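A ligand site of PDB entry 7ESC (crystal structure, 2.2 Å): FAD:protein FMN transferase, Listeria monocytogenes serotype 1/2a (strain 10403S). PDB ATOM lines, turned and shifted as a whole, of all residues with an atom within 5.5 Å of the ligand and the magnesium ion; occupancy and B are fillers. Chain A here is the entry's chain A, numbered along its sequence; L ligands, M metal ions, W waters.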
ATOM      1  N   SER A 106     -10.318  17.364 -19.480  1.00  0.00           N
ATOM      2  CA  SER A 106     -10.538  17.065 -18.043  1.00  0.00           C
ATOM      3  C   SER A 106     -12.015  17.233 -17.653  1.00  0.00           C
ATOM      4  O   SER A 106     -12.464  16.578 -16.682  1.00  0.00           O
ATOM      5  CB  SER A 106      -9.646  18.005 -17.256  1.00  0.00           C
ATOM      6  OG  SER A 106     -10.241  18.379 -16.031  1.00  0.00           O
ATOM      7  N   PHE A 107     -12.748  18.125 -18.325  1.00  0.00           N
ATOM      8  CA  PHE A 107     -14.149  18.469 -17.937  1.00  0.00           C
ATOM      9  C   PHE A 107     -15.109  17.974 -19.014  1.00  0.00           C
ATOM     10  O   PHE A 107     -14.825  18.177 -20.200  1.00  0.00           O
ATOM     11  CB  PHE A 107     -14.244  19.987 -17.732  1.00  0.00           C
ATOM     12  CG  PHE A 107     -15.594  20.480 -17.287  1.00  0.00           C
ATOM     13  CD1 PHE A 107     -15.855  20.587 -15.953  1.00  0.00           C
ATOM     14  CD2 PHE A 107     -16.569  20.862 -18.200  1.00  0.00           C
ATOM     15  CE1 PHE A 107     -17.086  21.074 -15.505  1.00  0.00           C
ATOM     16  CE2 PHE A 107     -17.804  21.319 -17.762  1.00  0.00           C
ATOM     17  CZ  PHE A 107     -18.059  21.434 -16.414  1.00  0.00           C
ATOM     18  N   ASP A 108     -16.190  17.314 -18.601  1.00  0.00           N
ATOM     19  CA  ASP A 108     -17.182  16.728 -19.544  1.00  0.00           C
ATOM     20  C   ASP A 108     -18.510  16.539 -18.827  1.00  0.00           C
ATOM     21  O   ASP A 108     -18.565  15.813 -17.831  1.00  0.00           O
ATOM     22  CB  ASP A 108     -16.654  15.409 -20.138  1.00  0.00           C
ATOM     23  CG  ASP A 108     -17.407  14.941 -21.365  1.00  0.00           C
ATOM     24  OD1 ASP A 108     -18.630  15.103 -21.386  1.00  0.00           O
ATOM     25  OD2 ASP A 108     -16.749  14.426 -22.285  1.00  0.00           O
ATOM     26  N   ILE A 109     -19.559  17.194 -19.293  1.00  0.00           N
ATOM     27  CA  ILE A 109     -20.875  17.088 -18.627  1.00  0.00           C
ATOM     28  C   ILE A 109     -21.495  15.713 -18.919  1.00  0.00           C
ATOM     29  O   ILE A 109     -22.476  15.342 -18.202  1.00  0.00           O
ATOM     30  CB  ILE A 109     -21.774  18.251 -19.072  1.00  0.00           C
ATOM     31  CG1 ILE A 109     -21.909  18.266 -20.591  1.00  0.00           C
ATOM     32  CG2 ILE A 109     -21.237  19.567 -18.551  1.00  0.00           C
ATOM     33  CD1 ILE A 109     -22.627  19.449 -21.093  1.00  0.00           C
ATOM     34  N   ILE A 111     -20.101  13.003 -18.127  1.00  0.00           N
ATOM     35  CA  ILE A 111     -19.413  12.100 -17.164  1.00  0.00           C
ATOM     36  C   ILE A 111     -20.472  11.370 -16.327  1.00  0.00           C
ATOM     37  O   ILE A 111     -20.115  10.614 -15.407  1.00  0.00           O
ATOM     38  CB  ILE A 111     -18.458  12.921 -16.287  1.00  0.00           C
ATOM     39  CG1 ILE A 111     -17.391  12.001 -15.668  1.00  0.00           C
ATOM     40  CG2 ILE A 111     -19.237  13.730 -15.257  1.00  0.00           C
ATOM     41  CD1 ILE A 111     -16.446  12.751 -14.776  1.00  0.00           C
ATOM     42  N   THR A 115     -20.107   9.169 -12.850  1.00  0.00           N
ATOM     43  CA  THR A 115     -20.446   9.817 -11.568  1.00  0.00           C
ATOM     44  C   THR A 115     -21.636   9.066 -10.961  1.00  0.00           C
ATOM     45  O   THR A 115     -21.725   9.011  -9.748  1.00  0.00           O
ATOM     46  CB  THR A 115     -20.706  11.312 -11.730  1.00  0.00           C
ATOM     47  OG1 THR A 115     -21.688  11.472 -12.770  1.00  0.00           O
ATOM     48  CG2 THR A 115     -19.423  12.040 -12.055  1.00  0.00           C
ATOM     49  N   ILE A 120     -20.382   9.314  -5.435  1.00  0.00           N
ATOM     50  CA  ILE A 120     -19.669   9.881  -4.246  1.00  0.00           C
ATOM     51  C   ILE A 120     -20.592  10.888  -3.555  1.00  0.00           C
ATOM     52  O   ILE A 120     -21.262  11.689  -4.258  1.00  0.00           O
ATOM     53  CB  ILE A 120     -18.325  10.490  -4.670  1.00  0.00           C
ATOM     54  CG1 ILE A 120     -17.404   9.426  -5.273  1.00  0.00           C
ATOM     55  CG2 ILE A 120     -17.659  11.198  -3.506  1.00  0.00           C
ATOM     56  CD1 ILE A 120     -16.261   9.982  -6.082  1.00  0.00           C
ATOM     57  N   ASP A 164     -24.425  15.085 -16.475  1.00  0.00           N
ATOM     58  CA  ASP A 164     -24.245  15.480 -15.055  1.00  0.00           C
ATOM     59  C   ASP A 164     -23.766  16.926 -15.081  1.00  0.00           C
ATOM     60  O   ASP A 164     -22.688  17.217 -15.646  1.00  0.00           O
ATOM     61  CB  ASP A 164     -23.300  14.501 -14.373  1.00  0.00           C
ATOM     62  CG  ASP A 164     -23.125  14.810 -12.897  1.00  0.00           C
ATOM     63  OD1 ASP A 164     -23.776  15.765 -12.422  1.00  0.00           O
ATOM     64  OD2 ASP A 164     -22.262  14.152 -12.261  1.00  0.00           O
ATOM     65  N   GLY A 166     -23.555  18.725 -12.165  1.00  0.00           N
ATOM     66  CA  GLY A 166     -23.216  19.008 -10.763  1.00  0.00           C
ATOM     67  C   GLY A 166     -22.048  19.983 -10.685  1.00  0.00           C
ATOM     68  O   GLY A 166     -21.998  20.723  -9.685  1.00  0.00           O
ATOM     69  N   ALA A 167     -21.117  19.942 -11.658  1.00  0.00           N
ATOM     70  CA  ALA A 167     -19.844  20.704 -11.568  1.00  0.00           C
ATOM     71  C   ALA A 167     -20.147  22.203 -11.758  1.00  0.00           C
ATOM     72  O   ALA A 167     -19.457  23.038 -11.173  1.00  0.00           O
ATOM     73  CB  ALA A 167     -18.824  20.153 -12.547  1.00  0.00           C
ATOM     74  N   ILE A 168     -21.176  22.563 -12.524  1.00  0.00           N
ATOM     75  CA  ILE A 168     -21.489  23.987 -12.814  1.00  0.00           C
ATOM     76  C   ILE A 168     -22.845  24.391 -12.255  1.00  0.00           C
ATOM     77  O   ILE A 168     -23.100  25.598 -12.350  1.00  0.00           O
ATOM     78  CB  ILE A 168     -21.429  24.317 -14.294  1.00  0.00           C
ATOM     79  CG1 ILE A 168     -22.332  23.370 -15.087  1.00  0.00           C
ATOM     80  CG2 ILE A 168     -20.002  24.263 -14.777  1.00  0.00           C
ATOM     81  CD1 ILE A 168     -22.083  23.492 -16.530  1.00  0.00           C
ATOM     82  N   VAL A 235     -15.163  30.118  -5.205  1.00  0.00           N
ATOM     83  CA  VAL A 235     -15.649  28.724  -5.331  1.00  0.00           C
ATOM     84  C   VAL A 235     -14.547  27.849  -4.779  1.00  0.00           C
ATOM     85  O   VAL A 235     -13.417  27.818  -5.327  1.00  0.00           O
ATOM     86  CB  VAL A 235     -15.990  28.349  -6.780  1.00  0.00           C
ATOM     87  CG1 VAL A 235     -16.340  26.838  -6.890  1.00  0.00           C
ATOM     88  CG2 VAL A 235     -17.095  29.215  -7.332  1.00  0.00           C
ATOM     89  N   SER A 237     -12.964  24.174  -3.682  1.00  0.00           N
ATOM     90  CA  SER A 237     -12.912  22.713  -3.945  1.00  0.00           C
ATOM     91  C   SER A 237     -11.948  22.079  -2.957  1.00  0.00           C
ATOM     92  O   SER A 237     -10.930  22.730  -2.630  1.00  0.00           O
ATOM     93  CB  SER A 237     -12.494  22.436  -5.360  1.00  0.00           C
ATOM     94  OG  SER A 237     -13.455  22.950  -6.283  1.00  0.00           O
ATOM     95  N   GLU A 241     -14.161  17.407   0.782  1.00  0.00           N
ATOM     96  CA  GLU A 241     -15.459  18.155   0.824  1.00  0.00           C
ATOM     97  C   GLU A 241     -16.594  17.125   0.820  1.00  0.00           C
ATOM     98  O   GLU A 241     -17.273  16.989   1.864  1.00  0.00           O
ATOM     99  CB  GLU A 241     -15.614  19.114  -0.354  1.00  0.00           C
ATOM    100  CG  GLU A 241     -16.907  19.912  -0.293  1.00  0.00           C
ATOM    101  CD  GLU A 241     -16.961  21.030  -1.315  1.00  0.00           C
ATOM    102  OE1 GLU A 241     -17.689  22.011  -1.089  1.00  0.00           O
ATOM    103  OE2 GLU A 241     -16.260  20.917  -2.334  1.00  0.00           O
ATOM    104  N   ARG A 242     -16.767  16.417  -0.281  1.00  0.00           N
ATOM    105  CA  ARG A 242     -17.652  15.217  -0.322  1.00  0.00           C
ATOM    106  C   ARG A 242     -16.814  14.058  -0.810  1.00  0.00           C
ATOM    107  O   ARG A 242     -16.431  14.072  -1.980  1.00  0.00           O
ATOM    108  CB  ARG A 242     -18.822  15.452  -1.262  1.00  0.00           C
ATOM    109  CG  ARG A 242     -20.029  16.153  -0.641  1.00  0.00           C
ATOM    110  CD  ARG A 242     -21.153  16.283  -1.669  1.00  0.00           C
ATOM    111  NE  ARG A 242     -20.656  16.854  -2.929  1.00  0.00           N
ATOM    112  CZ  ARG A 242     -20.437  16.194  -4.071  1.00  0.00           C
ATOM    113  NH1 ARG A 242     -20.690  14.893  -4.163  1.00  0.00           N
ATOM    114  NH2 ARG A 242     -19.958  16.843  -5.129  1.00  0.00           N
ATOM    115  N   HIS A 253     -14.836  13.815  -5.229  1.00  0.00           N
ATOM    116  CA  HIS A 253     -15.885  13.787  -6.283  1.00  0.00           C
ATOM    117  C   HIS A 253     -15.373  14.222  -7.657  1.00  0.00           C
ATOM    118  O   HIS A 253     -16.086  13.971  -8.642  1.00  0.00           O
ATOM    119  CB  HIS A 253     -17.079  14.620  -5.860  1.00  0.00           C
ATOM    120  CG  HIS A 253     -16.694  15.951  -5.327  1.00  0.00           C
ATOM    121  ND1 HIS A 253     -16.024  16.883  -6.109  1.00  0.00           N
ATOM    122  CD2 HIS A 253     -16.879  16.513  -4.117  1.00  0.00           C
ATOM    123  CE1 HIS A 253     -15.802  17.962  -5.382  1.00  0.00           C
ATOM    124  NE2 HIS A 253     -16.326  17.758  -4.153  1.00  0.00           N
ATOM    125  N   ILE A 254     -14.203  14.858  -7.743  1.00  0.00           N
ATOM    126  CA  ILE A 254     -13.686  15.330  -9.048  1.00  0.00           C
ATOM    127  C   ILE A 254     -12.976  14.180  -9.755  1.00  0.00           C
ATOM    128  O   ILE A 254     -11.847  13.885  -9.431  1.00  0.00           O
ATOM    129  CB  ILE A 254     -12.797  16.587  -8.906  1.00  0.00           C
ATOM    130  CG1 ILE A 254     -13.523  17.696  -8.121  1.00  0.00           C
ATOM    131  CG2 ILE A 254     -12.391  17.056 -10.290  1.00  0.00           C
ATOM    132  CD1 ILE A 254     -12.607  18.788  -7.576  1.00  0.00           C
ATOM    133  N   LEU A 255     -13.637  13.587 -10.732  1.00  0.00           N
ATOM    134  CA  LEU A 255     -13.167  12.365 -11.433  1.00  0.00           C
ATOM    135  C   LEU A 255     -12.506  12.730 -12.767  1.00  0.00           C
ATOM    136  O   LEU A 255     -12.856  13.783 -13.369  1.00  0.00           O
ATOM    137  CB  LEU A 255     -14.376  11.442 -11.649  1.00  0.00           C
ATOM    138  CG  LEU A 255     -15.234  11.133 -10.420  1.00  0.00           C
ATOM    139  CD1 LEU A 255     -16.274  10.091 -10.788  1.00  0.00           C
ATOM    140  CD2 LEU A 255     -14.399  10.655  -9.249  1.00  0.00           C
ATOM    141  N   ASP A 256     -11.592  11.871 -13.213  1.00  0.00           N
ATOM    142  CA  ASP A 256     -10.874  11.997 -14.514  1.00  0.00           C
ATOM    143  C   ASP A 256     -11.660  11.181 -15.513  1.00  0.00           C
ATOM    144  O   ASP A 256     -11.773   9.972 -15.369  1.00  0.00           O
ATOM    145  CB  ASP A 256      -9.428  11.480 -14.451  1.00  0.00           C
ATOM    146  CG  ASP A 256      -8.586  11.825 -15.673  1.00  0.00           C
ATOM    147  OD1 ASP A 256      -9.198  12.266 -16.656  1.00  0.00           O
ATOM    148  OD2 ASP A 256      -7.303  11.685 -15.618  1.00  0.00           O
ATOM    149  N   PRO A 257     -12.310  11.823 -16.501  1.00  0.00           N
ATOM    150  CA  PRO A 257     -13.177  11.091 -17.407  1.00  0.00           C
ATOM    151  C   PRO A 257     -12.405  10.043 -18.232  1.00  0.00           C
ATOM    152  O   PRO A 257     -13.024   9.142 -18.788  1.00  0.00           O
ATOM    153  CB  PRO A 257     -13.786  12.176 -18.301  1.00  0.00           C
ATOM    154  CG  PRO A 257     -12.872  13.351 -18.145  1.00  0.00           C
ATOM    155  CD  PRO A 257     -12.345  13.282 -16.722  1.00  0.00           C
ATOM    156  N   PHE A 263      -8.914  12.554  -9.487  1.00  0.00           N
ATOM    157  CA  PHE A 263      -7.624  13.215  -9.762  1.00  0.00           C
ATOM    158  C   PHE A 263      -6.828  13.214  -8.469  1.00  0.00           C
ATOM    159  O   PHE A 263      -7.411  13.435  -7.381  1.00  0.00           O
ATOM    160  CB  PHE A 263      -7.814  14.659 -10.193  1.00  0.00           C
ATOM    161  CG  PHE A 263      -8.256  14.807 -11.610  1.00  0.00           C
ATOM    162  CD1 PHE A 263      -7.384  14.503 -12.630  1.00  0.00           C
ATOM    163  CD2 PHE A 263      -9.557  15.218 -11.913  1.00  0.00           C
ATOM    164  CE1 PHE A 263      -7.804  14.598 -13.956  1.00  0.00           C
ATOM    165  CE2 PHE A 263      -9.951  15.366 -13.230  1.00  0.00           C
ATOM    166  CZ  PHE A 263      -9.078  15.041 -14.246  1.00  0.00           C
ATOM    167  N   ASP A 281     -16.858  27.592 -10.861  1.00  0.00           N
ATOM    168  CA  ASP A 281     -17.279  26.173 -10.909  1.00  0.00           C
ATOM    169  C   ASP A 281     -16.686  25.582 -12.187  1.00  0.00           C
ATOM    170  O   ASP A 281     -16.034  24.535 -12.084  1.00  0.00           O
ATOM    171  CB  ASP A 281     -18.780  25.961 -10.740  1.00  0.00           C
ATOM    172  CG  ASP A 281     -19.173  25.406  -9.384  1.00  0.00           C
ATOM    173  OD1 ASP A 281     -18.302  24.888  -8.668  1.00  0.00           O
ATOM    174  OD2 ASP A 281     -20.356  25.423  -9.066  1.00  0.00           O
ATOM    175  N   GLY A 282     -16.863  26.251 -13.316  1.00  0.00           N
ATOM    176  CA  GLY A 282     -16.462  25.711 -14.635  1.00  0.00           C
ATOM    177  C   GLY A 282     -14.970  25.431 -14.765  1.00  0.00           C
ATOM    178  O   GLY A 282     -14.642  24.429 -15.417  1.00  0.00           O
ATOM    179  N   SER A 284     -12.904  24.807 -12.300  1.00  0.00           N
ATOM    180  CA  SER A 284     -12.413  24.119 -11.073  1.00  0.00           C
ATOM    181  C   SER A 284     -11.774  22.785 -11.444  1.00  0.00           C
ATOM    182  O   SER A 284     -10.717  22.440 -10.922  1.00  0.00           O
ATOM    183  CB  SER A 284     -13.484  23.908 -10.056  1.00  0.00           C
ATOM    184  OG  SER A 284     -13.822  25.136  -9.441  1.00  0.00           O
ATOM    185  N   THR A 285     -12.445  22.032 -12.300  1.00  0.00           N
ATOM    186  CA  THR A 285     -12.034  20.675 -12.677  1.00  0.00           C
ATOM    187  C   THR A 285     -10.667  20.714 -13.362  1.00  0.00           C
ATOM    188  O   THR A 285      -9.733  19.979 -12.896  1.00  0.00           O
ATOM    189  CB  THR A 285     -13.114  20.017 -13.522  1.00  0.00           C
ATOM    190  OG1 THR A 285     -14.324  19.904 -12.756  1.00  0.00           O
ATOM    191  CG2 THR A 285     -12.618  18.669 -13.967  1.00  0.00           C
HETATM  192  P1  LIG L   1     -17.146  20.417  -7.662  1.00  0.00           P
HETATM  193  O1  LIG L   1     -17.586  21.812  -8.060  1.00  0.00           O
HETATM  194  O2  LIG L   1     -15.659  20.178  -7.953  1.00  0.00           O
HETATM  195  O3  LIG L   1     -17.533  20.086  -6.215  1.00  0.00           O
HETATM  196  O4  LIG L   1     -17.996  19.444  -8.666  1.00  0.00           O
HETATM  197  C1  LIG L   1     -18.082  18.031  -8.406  1.00  0.00           C
HETATM  198  C2  LIG L   1     -19.352  17.452  -9.013  1.00  0.00           C
HETATM  199  O5  LIG L   1     -19.349  17.661 -10.451  1.00  0.00           O
HETATM  200  C3  LIG L   1     -19.531  15.946  -8.831  1.00  0.00           C
HETATM  201  O6  LIG L   1     -20.438  15.660  -7.764  1.00  0.00           O
HETATM  202  C4  LIG L   1     -20.150  15.472 -10.153  1.00  0.00           C
HETATM  203  O7  LIG L   1     -21.549  15.591 -10.098  1.00  0.00           O
HETATM  204  C5  LIG L   1     -19.554  16.460 -11.152  1.00  0.00           C
HETATM  205  N1  LIG L   1     -18.270  16.070 -11.746  1.00  0.00           N
HETATM  206  C6  LIG L   1     -17.241  15.393 -11.148  1.00  0.00           C
HETATM  207  N2  LIG L   1     -16.188  15.261 -11.917  1.00  0.00           N
HETATM  208  C7  LIG L   1     -16.553  15.855 -13.101  1.00  0.00           C
HETATM  209  C8  LIG L   1     -15.876  16.042 -14.307  1.00  0.00           C
HETATM  210  N3  LIG L   1     -14.634  15.623 -14.509  1.00  0.00           N
HETATM  211  N4  LIG L   1     -16.516  16.701 -15.302  1.00  0.00           N
HETATM  212  C9  LIG L   1     -17.763  17.131 -15.068  1.00  0.00           C
HETATM  213  N5  LIG L   1     -18.507  17.012 -13.971  1.00  0.00           N
HETATM  214  C10 LIG L   1     -17.833  16.365 -13.004  1.00  0.00           C
HETATM  215 MG    MG M   1     -17.142  22.184 -10.220  1.00  0.00          MG
HETATM  216  O   HOH W   1     -20.977  18.290 -13.852  1.00  0.00           O
HETATM  217  O   HOH W   2     -15.194  22.395 -13.095  1.00  0.00           O
HETATM  218  O   HOH W   3     -24.683  16.169  -9.884  1.00  0.00           O
HETATM  219  O   HOH W   4     -18.493  12.908  -8.658  1.00  0.00           O
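A nitrogen (N4) of the ligand is in hydrogen-bond range of the backbone NH (N) of Asp 108 (3.4 Å).
O of Leu 255 sits at hydrogen-bond distance from N3 of the ligand, at 2.8 Å.
O of Ser 106 lies within hydrogen-bond range of N3 of the ligand (3.2 Å).
A nitrogen (N2) of the ligand sits at hydrogen-bond distance from the backbone NH (N) of Leu 255, 3.3 Å away.
N of Ala 167 is in hydrogen-bond range of O5 of the ligand (3.1 Å).
NE2 of His 253 sits close to O3 of the ligand (3.3 Å).
O6 of the ligand is in hydrogen-bond range of NH2 of Arg 242 (2.9 Å).
O7 of the ligand lies within hydrogen-bond range of OD2 of Asp 164 (2.7 Å).
NH1 of Arg 242 sits at hydrogen-bond distance from O of Ile 120.
The backbone carbonyl oxygen (O) of Ile 111 lies within hydrogen-bond range of the side-chain hydroxyl (OG1) of Thr 115 (3.2 Å).
N of Phe 263 lies within hydrogen-bond range of O of Ile 254 (3.2 Å).
The side-chain carboxylate (OD1) of Asp 164 sits at hydrogen-bond distance from the backbone NH (N) of Gly 166 (3.0 Å).
OG1 of Thr 115 lies within hydrogen-bond range of OD2 of Asp 164 (2.8 Å).
The backbone carbonyl oxygen (O) of Asp 281 sits close to the side-chain hydroxyl (OG) of Ser 284, 3.5 Å away.
N of Asp 164 is in hydrogen-bond range of O of Ile 109 (2.6 Å).
An oxygen (O1) of the ligand sits close to the side-chain carboxylate (OD1) of Asp 281, 3.2 Å away.
Merely in contact with the ligand: Ile 254, Ile 111, Gly 166, Thr 285, Ser 237, Pro 257, Phe 107 and Thr 115.
Hydrophobic or aromatic side chains that line the ligand: Phe 107, Ile 111, Ala 167, His 253, Ile 254 and Pro 257.
Of the 25 residues printed, 16 come within 4 Å of the ligand.
The nearest printed residue that does not touch the ligand is Glu 241 (4.2 Å).
Residues that only touch the magnesium ion: Asp 281 (3.2 Å).
Two residues have an atom within 4 Å of the magnesium ion: Ala 167 and Asp 281.
The nearest printed residue that does not touch the magnesium ion is Ser 284 (4.05 Å).
O1 of the ligand is bound to the magnesium ion (2.2 Å).
The magnesium ion has one donor atom within binding distance.
Slightly farther from the magnesium ion lies O of Ala 167 (2.6 Å).
Water W1 lies within hydrogen-bond range of O of Asp 164 (2.7 Å), N of Ala 167 (2.7 Å), N5 of the ligand (2.8 Å) and N of Gly 166 (3.1 Å).
Water W3 lies within hydrogen-bond range of OD1 of Asp 164 (2.7 Å) and O7 of the ligand (3.2 Å).
Water W4 lies within hydrogen-bond range of O of His 253 (2.6 Å) and O6 of the ligand (3.5 Å).
Water W2 lies within hydrogen-bond range of O of Asp 281, OG1 of Thr 285, O of Gly 282 and N of Ser 284.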
